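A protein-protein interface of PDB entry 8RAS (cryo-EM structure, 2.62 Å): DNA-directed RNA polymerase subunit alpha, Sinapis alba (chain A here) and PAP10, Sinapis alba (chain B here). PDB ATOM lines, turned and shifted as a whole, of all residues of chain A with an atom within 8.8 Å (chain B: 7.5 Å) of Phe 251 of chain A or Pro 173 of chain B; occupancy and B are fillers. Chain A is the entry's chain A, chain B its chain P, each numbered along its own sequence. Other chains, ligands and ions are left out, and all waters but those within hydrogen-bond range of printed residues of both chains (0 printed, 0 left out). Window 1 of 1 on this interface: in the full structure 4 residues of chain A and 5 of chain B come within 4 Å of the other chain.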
ATOM      1  N   PHE A 237      -5.531 -25.515 -23.550  1.00  0.00           N
ATOM      2  CA  PHE A 237      -5.085 -24.573 -22.538  1.00  0.00           C
ATOM      3  C   PHE A 237      -5.840 -24.825 -21.238  1.00  0.00           C
ATOM      4  O   PHE A 237      -6.937 -25.390 -21.230  1.00  0.00           O
ATOM      5  CB  PHE A 237      -5.308 -23.130 -23.001  1.00  0.00           C
ATOM      6  CG  PHE A 237      -4.571 -22.775 -24.262  1.00  0.00           C
ATOM      7  CD1 PHE A 237      -3.218 -23.033 -24.391  1.00  0.00           C
ATOM      8  CD2 PHE A 237      -5.236 -22.183 -25.321  1.00  0.00           C
ATOM      9  CE1 PHE A 237      -2.544 -22.707 -25.554  1.00  0.00           C
ATOM     10  CE2 PHE A 237      -4.566 -21.855 -26.483  1.00  0.00           C
ATOM     11  CZ  PHE A 237      -3.220 -22.117 -26.599  1.00  0.00           C
ATOM     12  N   TYR A 238      -5.234 -24.407 -20.131  1.00  0.00           N
ATOM     13  CA  TYR A 238      -5.874 -24.570 -18.834  1.00  0.00           C
ATOM     14  C   TYR A 238      -7.109 -23.684 -18.735  1.00  0.00           C
ATOM     15  O   TYR A 238      -7.106 -22.532 -19.178  1.00  0.00           O
ATOM     16  CB  TYR A 238      -4.896 -24.237 -17.707  1.00  0.00           C
ATOM     17  CG  TYR A 238      -5.487 -24.399 -16.324  1.00  0.00           C
ATOM     18  CD1 TYR A 238      -5.555 -25.647 -15.718  1.00  0.00           C
ATOM     19  CD2 TYR A 238      -5.977 -23.305 -15.624  1.00  0.00           C
ATOM     20  CE1 TYR A 238      -6.096 -25.799 -14.457  1.00  0.00           C
ATOM     21  CE2 TYR A 238      -6.520 -23.449 -14.363  1.00  0.00           C
ATOM     22  CZ  TYR A 238      -6.576 -24.698 -13.784  1.00  0.00           C
ATOM     23  OH  TYR A 238      -7.114 -24.844 -12.526  1.00  0.00           O
ATOM     24  N   LEU A 239      -8.170 -24.231 -18.152  1.00  0.00           N
ATOM     25  CA  LEU A 239      -9.413 -23.489 -17.973  1.00  0.00           C
ATOM     26  C   LEU A 239      -9.773 -23.374 -16.497  1.00  0.00           C
ATOM     27  O   LEU A 239     -10.336 -24.298 -15.912  1.00  0.00           O
ATOM     28  CB  LEU A 239     -10.553 -24.158 -18.743  1.00  0.00           C
ATOM     29  CG  LEU A 239     -10.821 -23.629 -20.153  1.00  0.00           C
ATOM     30  CD1 LEU A 239     -12.075 -24.263 -20.733  1.00  0.00           C
ATOM     31  CD2 LEU A 239     -10.940 -22.114 -20.141  1.00  0.00           C
ATOM     32  N   THR A 247     -10.996 -15.642 -24.057  1.00  0.00           N
ATOM     33  CA  THR A 247     -10.487 -14.382 -24.585  1.00  0.00           C
ATOM     34  C   THR A 247      -8.966 -14.333 -24.492  1.00  0.00           C
ATOM     35  O   THR A 247      -8.281 -14.127 -25.493  1.00  0.00           O
ATOM     36  CB  THR A 247     -11.083 -13.174 -23.836  1.00  0.00           C
ATOM     37  OG1 THR A 247     -12.503 -13.326 -23.732  1.00  0.00           O
ATOM     38  CG2 THR A 247     -10.772 -11.881 -24.574  1.00  0.00           C
ATOM     39  N   LEU A 248      -8.446 -14.520 -23.282  1.00  0.00           N
ATOM     40  CA  LEU A 248      -7.006 -14.540 -23.030  1.00  0.00           C
ATOM     41  C   LEU A 248      -6.657 -15.825 -22.291  1.00  0.00           C
ATOM     42  O   LEU A 248      -6.778 -15.883 -21.054  1.00  0.00           O
ATOM     43  CB  LEU A 248      -6.566 -13.316 -22.236  1.00  0.00           C
ATOM     44  CG  LEU A 248      -6.895 -11.967 -22.876  1.00  0.00           C
ATOM     45  CD1 LEU A 248      -6.835 -10.858 -21.846  1.00  0.00           C
ATOM     46  CD2 LEU A 248      -5.953 -11.678 -24.035  1.00  0.00           C
ATOM     47  N   PRO A 249      -6.230 -16.869 -23.003  1.00  0.00           N
ATOM     48  CA  PRO A 249      -5.949 -18.152 -22.336  1.00  0.00           C
ATOM     49  C   PRO A 249      -4.819 -18.089 -21.320  1.00  0.00           C
ATOM     50  O   PRO A 249      -4.730 -18.977 -20.465  1.00  0.00           O
ATOM     51  CB  PRO A 249      -5.595 -19.087 -23.502  1.00  0.00           C
ATOM     52  CG  PRO A 249      -5.232 -18.183 -24.634  1.00  0.00           C
ATOM     53  CD  PRO A 249      -6.051 -16.945 -24.462  1.00  0.00           C
ATOM     54  N   LEU A 250      -3.950 -17.079 -21.394  1.00  0.00           N
ATOM     55  CA  LEU A 250      -2.841 -16.980 -20.450  1.00  0.00           C
ATOM     56  C   LEU A 250      -3.335 -16.754 -19.025  1.00  0.00           C
ATOM     57  O   LEU A 250      -2.795 -17.330 -18.073  1.00  0.00           O
ATOM     58  CB  LEU A 250      -1.903 -15.849 -20.872  1.00  0.00           C
ATOM     59  CG  LEU A 250      -0.616 -15.675 -20.067  1.00  0.00           C
ATOM     60  CD1 LEU A 250       0.500 -16.500 -20.666  1.00  0.00           C
ATOM     61  CD2 LEU A 250      -0.225 -14.213 -20.003  1.00  0.00           C
ATOM     62  N   PHE A 251      -4.354 -15.913 -18.862  1.00  0.00           N
ATOM     63  CA  PHE A 251      -4.754 -15.468 -17.529  1.00  0.00           C
ATOM     64  C   PHE A 251      -5.252 -16.580 -16.606  1.00  0.00           C
ATOM     65  O   PHE A 251      -4.887 -16.554 -15.416  1.00  0.00           O
ATOM     66  CB  PHE A 251      -5.799 -14.354 -17.662  1.00  0.00           C
ATOM     67  CG  PHE A 251      -5.213 -13.019 -18.036  1.00  0.00           C
ATOM     68  CD1 PHE A 251      -3.848 -12.874 -18.218  1.00  0.00           C
ATOM     69  CD2 PHE A 251      -6.026 -11.914 -18.209  1.00  0.00           C
ATOM     70  CE1 PHE A 251      -3.306 -11.652 -18.561  1.00  0.00           C
ATOM     71  CE2 PHE A 251      -5.489 -10.689 -18.550  1.00  0.00           C
ATOM     72  CZ  PHE A 251      -4.128 -10.559 -18.727  1.00  0.00           C
ATOM     73  N   PRO A 252      -6.092 -17.533 -17.038  1.00  0.00           N
ATOM     74  CA  PRO A 252      -6.506 -18.594 -16.100  1.00  0.00           C
ATOM     75  C   PRO A 252      -5.345 -19.398 -15.538  1.00  0.00           C
ATOM     76  O   PRO A 252      -5.369 -19.769 -14.356  1.00  0.00           O
ATOM     77  CB  PRO A 252      -7.448 -19.467 -16.945  1.00  0.00           C
ATOM     78  CG  PRO A 252      -7.191 -19.078 -18.361  1.00  0.00           C
ATOM     79  CD  PRO A 252      -6.816 -17.638 -18.316  1.00  0.00           C
ATOM     80  N   PHE A 253      -4.316 -19.670 -16.342  1.00  0.00           N
ATOM     81  CA  PHE A 253      -3.158 -20.385 -15.816  1.00  0.00           C
ATOM     82  C   PHE A 253      -2.374 -19.528 -14.832  1.00  0.00           C
ATOM     83  O   PHE A 253      -1.821 -20.053 -13.860  1.00  0.00           O
ATOM     84  CB  PHE A 253      -2.255 -20.852 -16.955  1.00  0.00           C
ATOM     85  CG  PHE A 253      -1.197 -21.829 -16.526  1.00  0.00           C
ATOM     86  CD1 PHE A 253      -1.484 -23.180 -16.433  1.00  0.00           C
ATOM     87  CD2 PHE A 253       0.081 -21.398 -16.216  1.00  0.00           C
ATOM     88  CE1 PHE A 253      -0.515 -24.083 -16.040  1.00  0.00           C
ATOM     89  CE2 PHE A 253       1.052 -22.297 -15.822  1.00  0.00           C
ATOM     90  CZ  PHE A 253       0.754 -23.642 -15.734  1.00  0.00           C
ATOM     91  N   HIS A 254      -2.311 -18.214 -15.061  1.00  0.00           N
ATOM     92  CA  HIS A 254      -1.689 -17.332 -14.080  1.00  0.00           C
ATOM     93  C   HIS A 254      -2.461 -17.346 -12.769  1.00  0.00           C
ATOM     94  O   HIS A 254      -1.863 -17.323 -11.688  1.00  0.00           O
ATOM     95  CB  HIS A 254      -1.594 -15.909 -14.629  1.00  0.00           C
ATOM     96  CG  HIS A 254      -1.255 -14.886 -13.590  1.00  0.00           C
ATOM     97  ND1 HIS A 254       0.040 -14.622 -13.201  1.00  0.00           N
ATOM     98  CD2 HIS A 254      -2.044 -14.069 -12.853  1.00  0.00           C
ATOM     99  CE1 HIS A 254       0.035 -13.682 -12.273  1.00  0.00           C
ATOM    100  NE2 HIS A 254      -1.216 -13.329 -12.044  1.00  0.00           N
ATOM    101  N   ASN A 255      -3.795 -17.372 -12.843  1.00  0.00           N
ATOM    102  CA  ASN A 255      -4.602 -17.485 -11.632  1.00  0.00           C
ATOM    103  C   ASN A 255      -4.340 -18.807 -10.921  1.00  0.00           C
ATOM    104  O   ASN A 255      -4.269 -18.857  -9.686  1.00  0.00           O
ATOM    105  CB  ASN A 255      -6.083 -17.343 -11.973  1.00  0.00           C
ATOM    106  CG  ASN A 255      -6.976 -17.488 -10.758  1.00  0.00           C
ATOM    107  OD1 ASN A 255      -7.816 -18.385 -10.694  1.00  0.00           O
ATOM    108  ND2 ASN A 255      -6.798 -16.604  -9.784  1.00  0.00           N
ATOM    109  N   LYS A 256      -4.205 -19.890 -11.688  1.00  0.00           N
ATOM    110  CA  LYS A 256      -3.873 -21.182 -11.095  1.00  0.00           C
ATOM    111  C   LYS A 256      -2.521 -21.137 -10.392  1.00  0.00           C
ATOM    112  O   LYS A 256      -2.368 -21.667  -9.287  1.00  0.00           O
ATOM    113  CB  LYS A 256      -3.881 -22.268 -12.169  1.00  0.00           C
ATOM    114  CG  LYS A 256      -3.452 -23.633 -11.667  1.00  0.00           C
ATOM    115  CD  LYS A 256      -2.825 -24.458 -12.775  1.00  0.00           C
ATOM    116  CE  LYS A 256      -2.260 -25.755 -12.233  1.00  0.00           C
ATOM    117  NZ  LYS A 256      -3.219 -26.438 -11.320  1.00  0.00           N
ATOM    118  N   LEU A 257      -1.526 -20.508 -11.023  1.00  0.00           N
ATOM    119  CA  LEU A 257      -0.214 -20.370 -10.396  1.00  0.00           C
ATOM    120  C   LEU A 257      -0.292 -19.530  -9.127  1.00  0.00           C
ATOM    121  O   LEU A 257       0.367 -19.838  -8.127  1.00  0.00           O
ATOM    122  CB  LEU A 257       0.776 -19.751 -11.381  1.00  0.00           C
ATOM    123  CG  LEU A 257       1.303 -20.644 -12.503  1.00  0.00           C
ATOM    124  CD1 LEU A 257       2.045 -19.805 -13.526  1.00  0.00           C
ATOM    125  CD2 LEU A 257       2.200 -21.737 -11.949  1.00  0.00           C
ATOM    126  N   VAL A 258      -1.085 -18.457  -9.157  1.00  0.00           N
ATOM    127  CA  VAL A 258      -1.254 -17.613  -7.977  1.00  0.00           C
ATOM    128  C   VAL A 258      -1.867 -18.413  -6.835  1.00  0.00           C
ATOM    129  O   VAL A 258      -1.422 -18.325  -5.684  1.00  0.00           O
ATOM    130  CB  VAL A 258      -2.106 -16.378  -8.327  1.00  0.00           C
ATOM    131  CG1 VAL A 258      -2.759 -15.800  -7.080  1.00  0.00           C
ATOM    132  CG2 VAL A 258      -1.258 -15.332  -9.032  1.00  0.00           C
ATOM    133  N   LEU B 113      -8.589  -3.621 -23.595  1.00  0.00           N
ATOM    134  CA  LEU B 113      -8.609  -4.660 -22.568  1.00  0.00           C
ATOM    135  C   LEU B 113      -7.967  -4.169 -21.272  1.00  0.00           C
ATOM    136  O   LEU B 113      -8.476  -4.432 -20.173  1.00  0.00           O
ATOM    137  CB  LEU B 113      -7.906  -5.915 -23.085  1.00  0.00           C
ATOM    138  CG  LEU B 113      -8.590  -6.622 -24.258  1.00  0.00           C
ATOM    139  CD1 LEU B 113      -7.613  -7.512 -25.009  1.00  0.00           C
ATOM    140  CD2 LEU B 113      -9.788  -7.424 -23.777  1.00  0.00           C
ATOM    141  N   MET B 114      -6.852  -3.444 -21.383  1.00  0.00           N
ATOM    142  CA  MET B 114      -6.223  -2.852 -20.209  1.00  0.00           C
ATOM    143  C   MET B 114      -7.115  -1.799 -19.574  1.00  0.00           C
ATOM    144  O   MET B 114      -7.099  -1.631 -18.353  1.00  0.00           O
ATOM    145  CB  MET B 114      -4.872  -2.247 -20.589  1.00  0.00           C
ATOM    146  CG  MET B 114      -4.073  -1.715 -19.411  1.00  0.00           C
ATOM    147  SD  MET B 114      -3.915  -2.929 -18.089  1.00  0.00           S
ATOM    148  CE  MET B 114      -2.411  -3.764 -18.583  1.00  0.00           C
ATOM    149  N   GLU B 117      -9.505  -3.744 -17.477  1.00  0.00           N
ATOM    150  CA  GLU B 117      -8.824  -4.204 -16.269  1.00  0.00           C
ATOM    151  C   GLU B 117      -8.625  -3.063 -15.278  1.00  0.00           C
ATOM    152  O   GLU B 117      -8.834  -3.233 -14.071  1.00  0.00           O
ATOM    153  CB  GLU B 117      -7.480  -4.837 -16.631  1.00  0.00           C
ATOM    154  CG  GLU B 117      -7.569  -6.295 -17.045  1.00  0.00           C
ATOM    155  CD  GLU B 117      -6.207  -6.948 -17.180  1.00  0.00           C
ATOM    156  OE1 GLU B 117      -5.277  -6.288 -17.685  1.00  0.00           O
ATOM    157  OE2 GLU B 117      -6.065  -8.121 -16.778  1.00  0.00           O
ATOM    158  N   LEU B 154       1.890   0.755 -18.441  1.00  0.00           N
ATOM    159  CA  LEU B 154       1.443   1.337 -17.184  1.00  0.00           C
ATOM    160  C   LEU B 154       2.646   1.815 -16.387  1.00  0.00           C
ATOM    161  O   LEU B 154       3.701   1.174 -16.391  1.00  0.00           O
ATOM    162  CB  LEU B 154       0.647   0.331 -16.351  1.00  0.00           C
ATOM    163  CG  LEU B 154      -0.540  -0.357 -17.019  1.00  0.00           C
ATOM    164  CD1 LEU B 154      -1.130  -1.376 -16.070  1.00  0.00           C
ATOM    165  CD2 LEU B 154      -1.585   0.658 -17.441  1.00  0.00           C
ATOM    166  N   PHE B 156       3.553   2.919 -12.460  1.00  0.00           N
ATOM    167  CA  PHE B 156       3.152   2.965 -11.059  1.00  0.00           C
ATOM    168  C   PHE B 156       4.061   3.955 -10.344  1.00  0.00           C
ATOM    169  O   PHE B 156       5.236   3.664 -10.098  1.00  0.00           O
ATOM    170  CB  PHE B 156       3.232   1.579 -10.421  1.00  0.00           C
ATOM    171  CG  PHE B 156       2.181   0.624 -10.910  1.00  0.00           C
ATOM    172  CD1 PHE B 156       2.271   0.056 -12.171  1.00  0.00           C
ATOM    173  CD2 PHE B 156       1.105   0.289 -10.107  1.00  0.00           C
ATOM    174  CE1 PHE B 156       1.305  -0.824 -12.620  1.00  0.00           C
ATOM    175  CE2 PHE B 156       0.138  -0.590 -10.551  1.00  0.00           C
ATOM    176  CZ  PHE B 156       0.238  -1.147 -11.809  1.00  0.00           C
ATOM    177  N   GLY B 170       2.792  -4.579 -21.642  1.00  0.00           N
ATOM    178  CA  GLY B 170       1.896  -5.653 -22.025  1.00  0.00           C
ATOM    179  C   GLY B 170       0.648  -5.703 -21.166  1.00  0.00           C
ATOM    180  O   GLY B 170       0.450  -4.922 -20.231  1.00  0.00           O
ATOM    181  N   LEU B 171      -0.210  -6.663 -21.512  1.00  0.00           N
ATOM    182  CA  LEU B 171      -1.491  -6.857 -20.835  1.00  0.00           C
ATOM    183  C   LEU B 171      -1.273  -7.767 -19.631  1.00  0.00           C
ATOM    184  O   LEU B 171      -1.533  -8.972 -19.660  1.00  0.00           O
ATOM    185  CB  LEU B 171      -2.517  -7.432 -21.802  1.00  0.00           C
ATOM    186  CG  LEU B 171      -3.991  -7.256 -21.450  1.00  0.00           C
ATOM    187  CD1 LEU B 171      -4.315  -5.793 -21.245  1.00  0.00           C
ATOM    188  CD2 LEU B 171      -4.856  -7.848 -22.545  1.00  0.00           C
ATOM    189  N   ILE B 172      -0.783  -7.170 -18.551  1.00  0.00           N
ATOM    190  CA  ILE B 172      -0.489  -7.905 -17.324  1.00  0.00           C
ATOM    191  C   ILE B 172      -1.792  -8.194 -16.586  1.00  0.00           C
ATOM    192  O   ILE B 172      -2.758  -7.430 -16.715  1.00  0.00           O
ATOM    193  CB  ILE B 172       0.497  -7.130 -16.435  1.00  0.00           C
ATOM    194  CG1 ILE B 172      -0.072  -5.757 -16.074  1.00  0.00           C
ATOM    195  CG2 ILE B 172       1.837  -6.985 -17.137  1.00  0.00           C
ATOM    196  CD1 ILE B 172       0.470  -5.196 -14.783  1.00  0.00           C
ATOM    197  N   PRO B 173      -1.868  -9.277 -15.819  1.00  0.00           N
ATOM    198  CA  PRO B 173      -3.098  -9.576 -15.078  1.00  0.00           C
ATOM    199  C   PRO B 173      -3.261  -8.663 -13.872  1.00  0.00           C
ATOM    200  O   PRO B 173      -2.346  -7.953 -13.452  1.00  0.00           O
ATOM    201  CB  PRO B 173      -2.915 -11.035 -14.655  1.00  0.00           C
ATOM    202  CG  PRO B 173      -1.446 -11.235 -14.631  1.00  0.00           C
ATOM    203  CD  PRO B 173      -0.866 -10.347 -15.686  1.00  0.00           C
ATOM    204  N   LEU B 174      -4.473  -8.694 -13.312  1.00  0.00           N
ATOM    205  CA  LEU B 174      -4.798  -7.838 -12.175  1.00  0.00           C
ATOM    206  C   LEU B 174      -4.019  -8.226 -10.926  1.00  0.00           C
ATOM    207  O   LEU B 174      -3.719  -7.362 -10.091  1.00  0.00           O
ATOM    208  CB  LEU B 174      -6.298  -7.897 -11.897  1.00  0.00           C
ATOM    209  CG  LEU B 174      -7.146  -6.801 -12.535  1.00  0.00           C
ATOM    210  CD1 LEU B 174      -8.614  -7.085 -12.313  1.00  0.00           C
ATOM    211  CD2 LEU B 174      -6.773  -5.447 -11.968  1.00  0.00           C
ATOM    212  N   GLN B 175      -3.696  -9.511 -10.773  1.00  0.00           N
ATOM    213  CA  GLN B 175      -2.972  -9.954  -9.586  1.00  0.00           C
ATOM    214  C   GLN B 175      -1.587  -9.327  -9.519  1.00  0.00           C
ATOM    215  O   GLN B 175      -1.107  -8.989  -8.433  1.00  0.00           O
ATOM    216  CB  GLN B 175      -2.876 -11.478  -9.562  1.00  0.00           C
ATOM    217  CG  GLN B 175      -2.508 -12.043  -8.200  1.00  0.00           C
ATOM    218  CD  GLN B 175      -3.319 -11.429  -7.075  1.00  0.00           C
ATOM    219  OE1 GLN B 175      -4.549 -11.402  -7.123  1.00  0.00           O
ATOM    220  NE2 GLN B 175      -2.631 -10.932  -6.055  1.00  0.00           N
ATOM    221  N   MET B 176      -0.927  -9.168 -10.667  1.00  0.00           N
ATOM    222  CA  MET B 176       0.358  -8.475 -10.690  1.00  0.00           C
ATOM    223  C   MET B 176       0.205  -7.025 -10.246  1.00  0.00           C
ATOM    224  O   MET B 176       1.048  -6.501  -9.508  1.00  0.00           O
ATOM    225  CB  MET B 176       0.963  -8.543 -12.090  1.00  0.00           C
ATOM    226  CG  MET B 176       1.942  -9.683 -12.290  1.00  0.00           C
ATOM    227  SD  MET B 176       3.004  -9.416 -13.721  1.00  0.00           S
ATOM    228  CE  MET B 176       3.106  -7.631 -13.736  1.00  0.00           C
ATOM    229  N   MET B 177      -0.862  -6.364 -10.694  1.00  0.00           N
ATOM    230  CA  MET B 177      -1.135  -4.994 -10.277  1.00  0.00           C
ATOM    231  C   MET B 177      -1.293  -4.910  -8.763  1.00  0.00           C
ATOM    232  O   MET B 177      -0.689  -4.053  -8.102  1.00  0.00           O
ATOM    233  CB  MET B 177      -2.404  -4.502 -10.972  1.00  0.00           C
ATOM    234  CG  MET B 177      -2.202  -4.014 -12.390  1.00  0.00           C
ATOM    235  SD  MET B 177      -3.656  -4.384 -13.389  1.00  0.00           S
ATOM    236  CE  MET B 177      -3.851  -2.868 -14.309  1.00  0.00           C
ATOM    237  N   ARG B 178      -2.106  -5.806  -8.199  1.00  0.00           N
ATOM    238  CA  ARG B 178      -2.328  -5.812  -6.758  1.00  0.00           C
ATOM    239  C   ARG B 178      -1.041  -6.116  -6.003  1.00  0.00           C
ATOM    240  O   ARG B 178      -0.771  -5.516  -4.958  1.00  0.00           O
ATOM    241  CB  ARG B 178      -3.416  -6.824  -6.403  1.00  0.00           C
ATOM    242  CG  ARG B 178      -4.751  -6.545  -7.068  1.00  0.00           C
ATOM    243  CD  ARG B 178      -5.863  -7.378  -6.457  1.00  0.00           C
ATOM    244  NE  ARG B 178      -6.121  -8.587  -7.230  1.00  0.00           N
ATOM    245  CZ  ARG B 178      -7.267  -8.855  -7.841  1.00  0.00           C
ATOM    246  NH1 ARG B 178      -8.287  -8.014  -7.795  1.00  0.00           N
ATOM    247  NH2 ARG B 178      -7.392  -9.994  -8.517  1.00  0.00           N
ATOM    248  N   ASP B 179      -0.236  -7.049  -6.516  1.00  0.00           N
ATOM    249  CA  ASP B 179       1.027  -7.380  -5.866  1.00  0.00           C
ATOM    250  C   ASP B 179       1.973  -6.188  -5.861  1.00  0.00           C
ATOM    251  O   ASP B 179       2.625  -5.910  -4.850  1.00  0.00           O
ATOM    252  CB  ASP B 179       1.674  -8.577  -6.562  1.00  0.00           C
ATOM    253  CG  ASP B 179       1.045  -9.893  -6.157  1.00  0.00           C
ATOM    254  OD1 ASP B 179      -0.061  -9.869  -5.577  1.00  0.00           O
ATOM    255  OD2 ASP B 179       1.657 -10.950  -6.415  1.00  0.00           O
ATOM    256  N   ILE B 180       2.060  -5.469  -6.982  1.00  0.00           N
ATOM    257  CA  ILE B 180       2.905  -4.278  -7.033  1.00  0.00           C
ATOM    258  C   ILE B 180       2.421  -3.247  -6.022  1.00  0.00           C
ATOM    259  O   ILE B 180       3.211  -2.696  -5.243  1.00  0.00           O
ATOM    260  CB  ILE B 180       2.936  -3.699  -8.459  1.00  0.00           C
ATOM    261  CG1 ILE B 180       3.643  -4.664  -9.412  1.00  0.00           C
ATOM    262  CG2 ILE B 180       3.613  -2.339  -8.472  1.00  0.00           C
ATOM    263  CD1 ILE B 180       3.467  -4.315 -10.872  1.00  0.00           C
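OE1 of Gln 175 of chain B sits at hydrogen-bond distance from NE of Arg 178 of chain B, 3.2 Å away. The side-chain amide nitrogen (NE2) of Gln 175 of chain B lies within hydrogen-bond range of the side-chain carboxylate (OD1) of Asp 179 of chain B (2.8 Å).
CD1 of Leu 248 of chain A touches CD2 of Leu 171 of chain B, at 3.7 Å. Glu 117 of chain B touches Phe 251 of chain A. Leu 171 of chain B touches Phe 251 of chain A. Ile 172 of chain B touches Phe 251 of chain A (C to CZ, 3.95 Å). Phe 251 of chain A touches Pro 173 of chain B. NE2 of His 254 of chain A touches CG of Pro 173 of chain B, 3.3 Å away. His 254 of chain A touches Gln 175 of chain B (NE2 to CB, 3.5 Å). Val 258 of chain A touches Gln 175 of chain B (CG2 to CG, 3.6 Å).
Phe 251 of chain A touches just these residues of chain B: Glu 117 (3.2 Å), Leu 171 (3.2 Å), Ile 172 (3.95 Å) and Pro 173 (3.9 Å). Met 114 of chain B touches none of the printed residues of chain A. Printed residues of chain A within 4 Å of Glu 117 of chain B: Phe 251. Of the printed residues of chain A, Leu 171 of chain B touches Leu 248 (3.7 Å) and Phe 251 (3.2 Å). Of chain A, only Phe 251 (3.95 Å) comes within 4 Å of Ile 172 of chain B. Pro 173 of chain B touches just these residues of chain A: Phe 251 (3.9 Å) and His 254 (3.3 Å). Printed residues of chain A within 4 Å of Gln 175 of chain B: His 254 (3.5 Å) and Val 258 (3.6 Å). The nearest residue of chain B that does not touch Phe 251 of chain A is Leu 174 of chain B (5.7 Å). The nearest printed residue of chain B that does not touch Val 258 of chain A is Asp 179 of chain B (5.9 Å).
Of the 15 printed residues of chain A, 4 touch a printed residue of chain B. Hydrophobic or aromatic side chains of chain A that line the printed part of chain B: Leu 248, Phe 251, His 254 and Val 258. Hydrophobic or aromatic side chains of chain B that line the printed part of chain A: Leu 171 and Pro 173. Among the printed residues, 8 pairs touch across the chains. Among the printed residues, no Asp or Glu carboxylate lies within 4 Å of a Lys or Arg side-chain nitrogen of the other chain.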
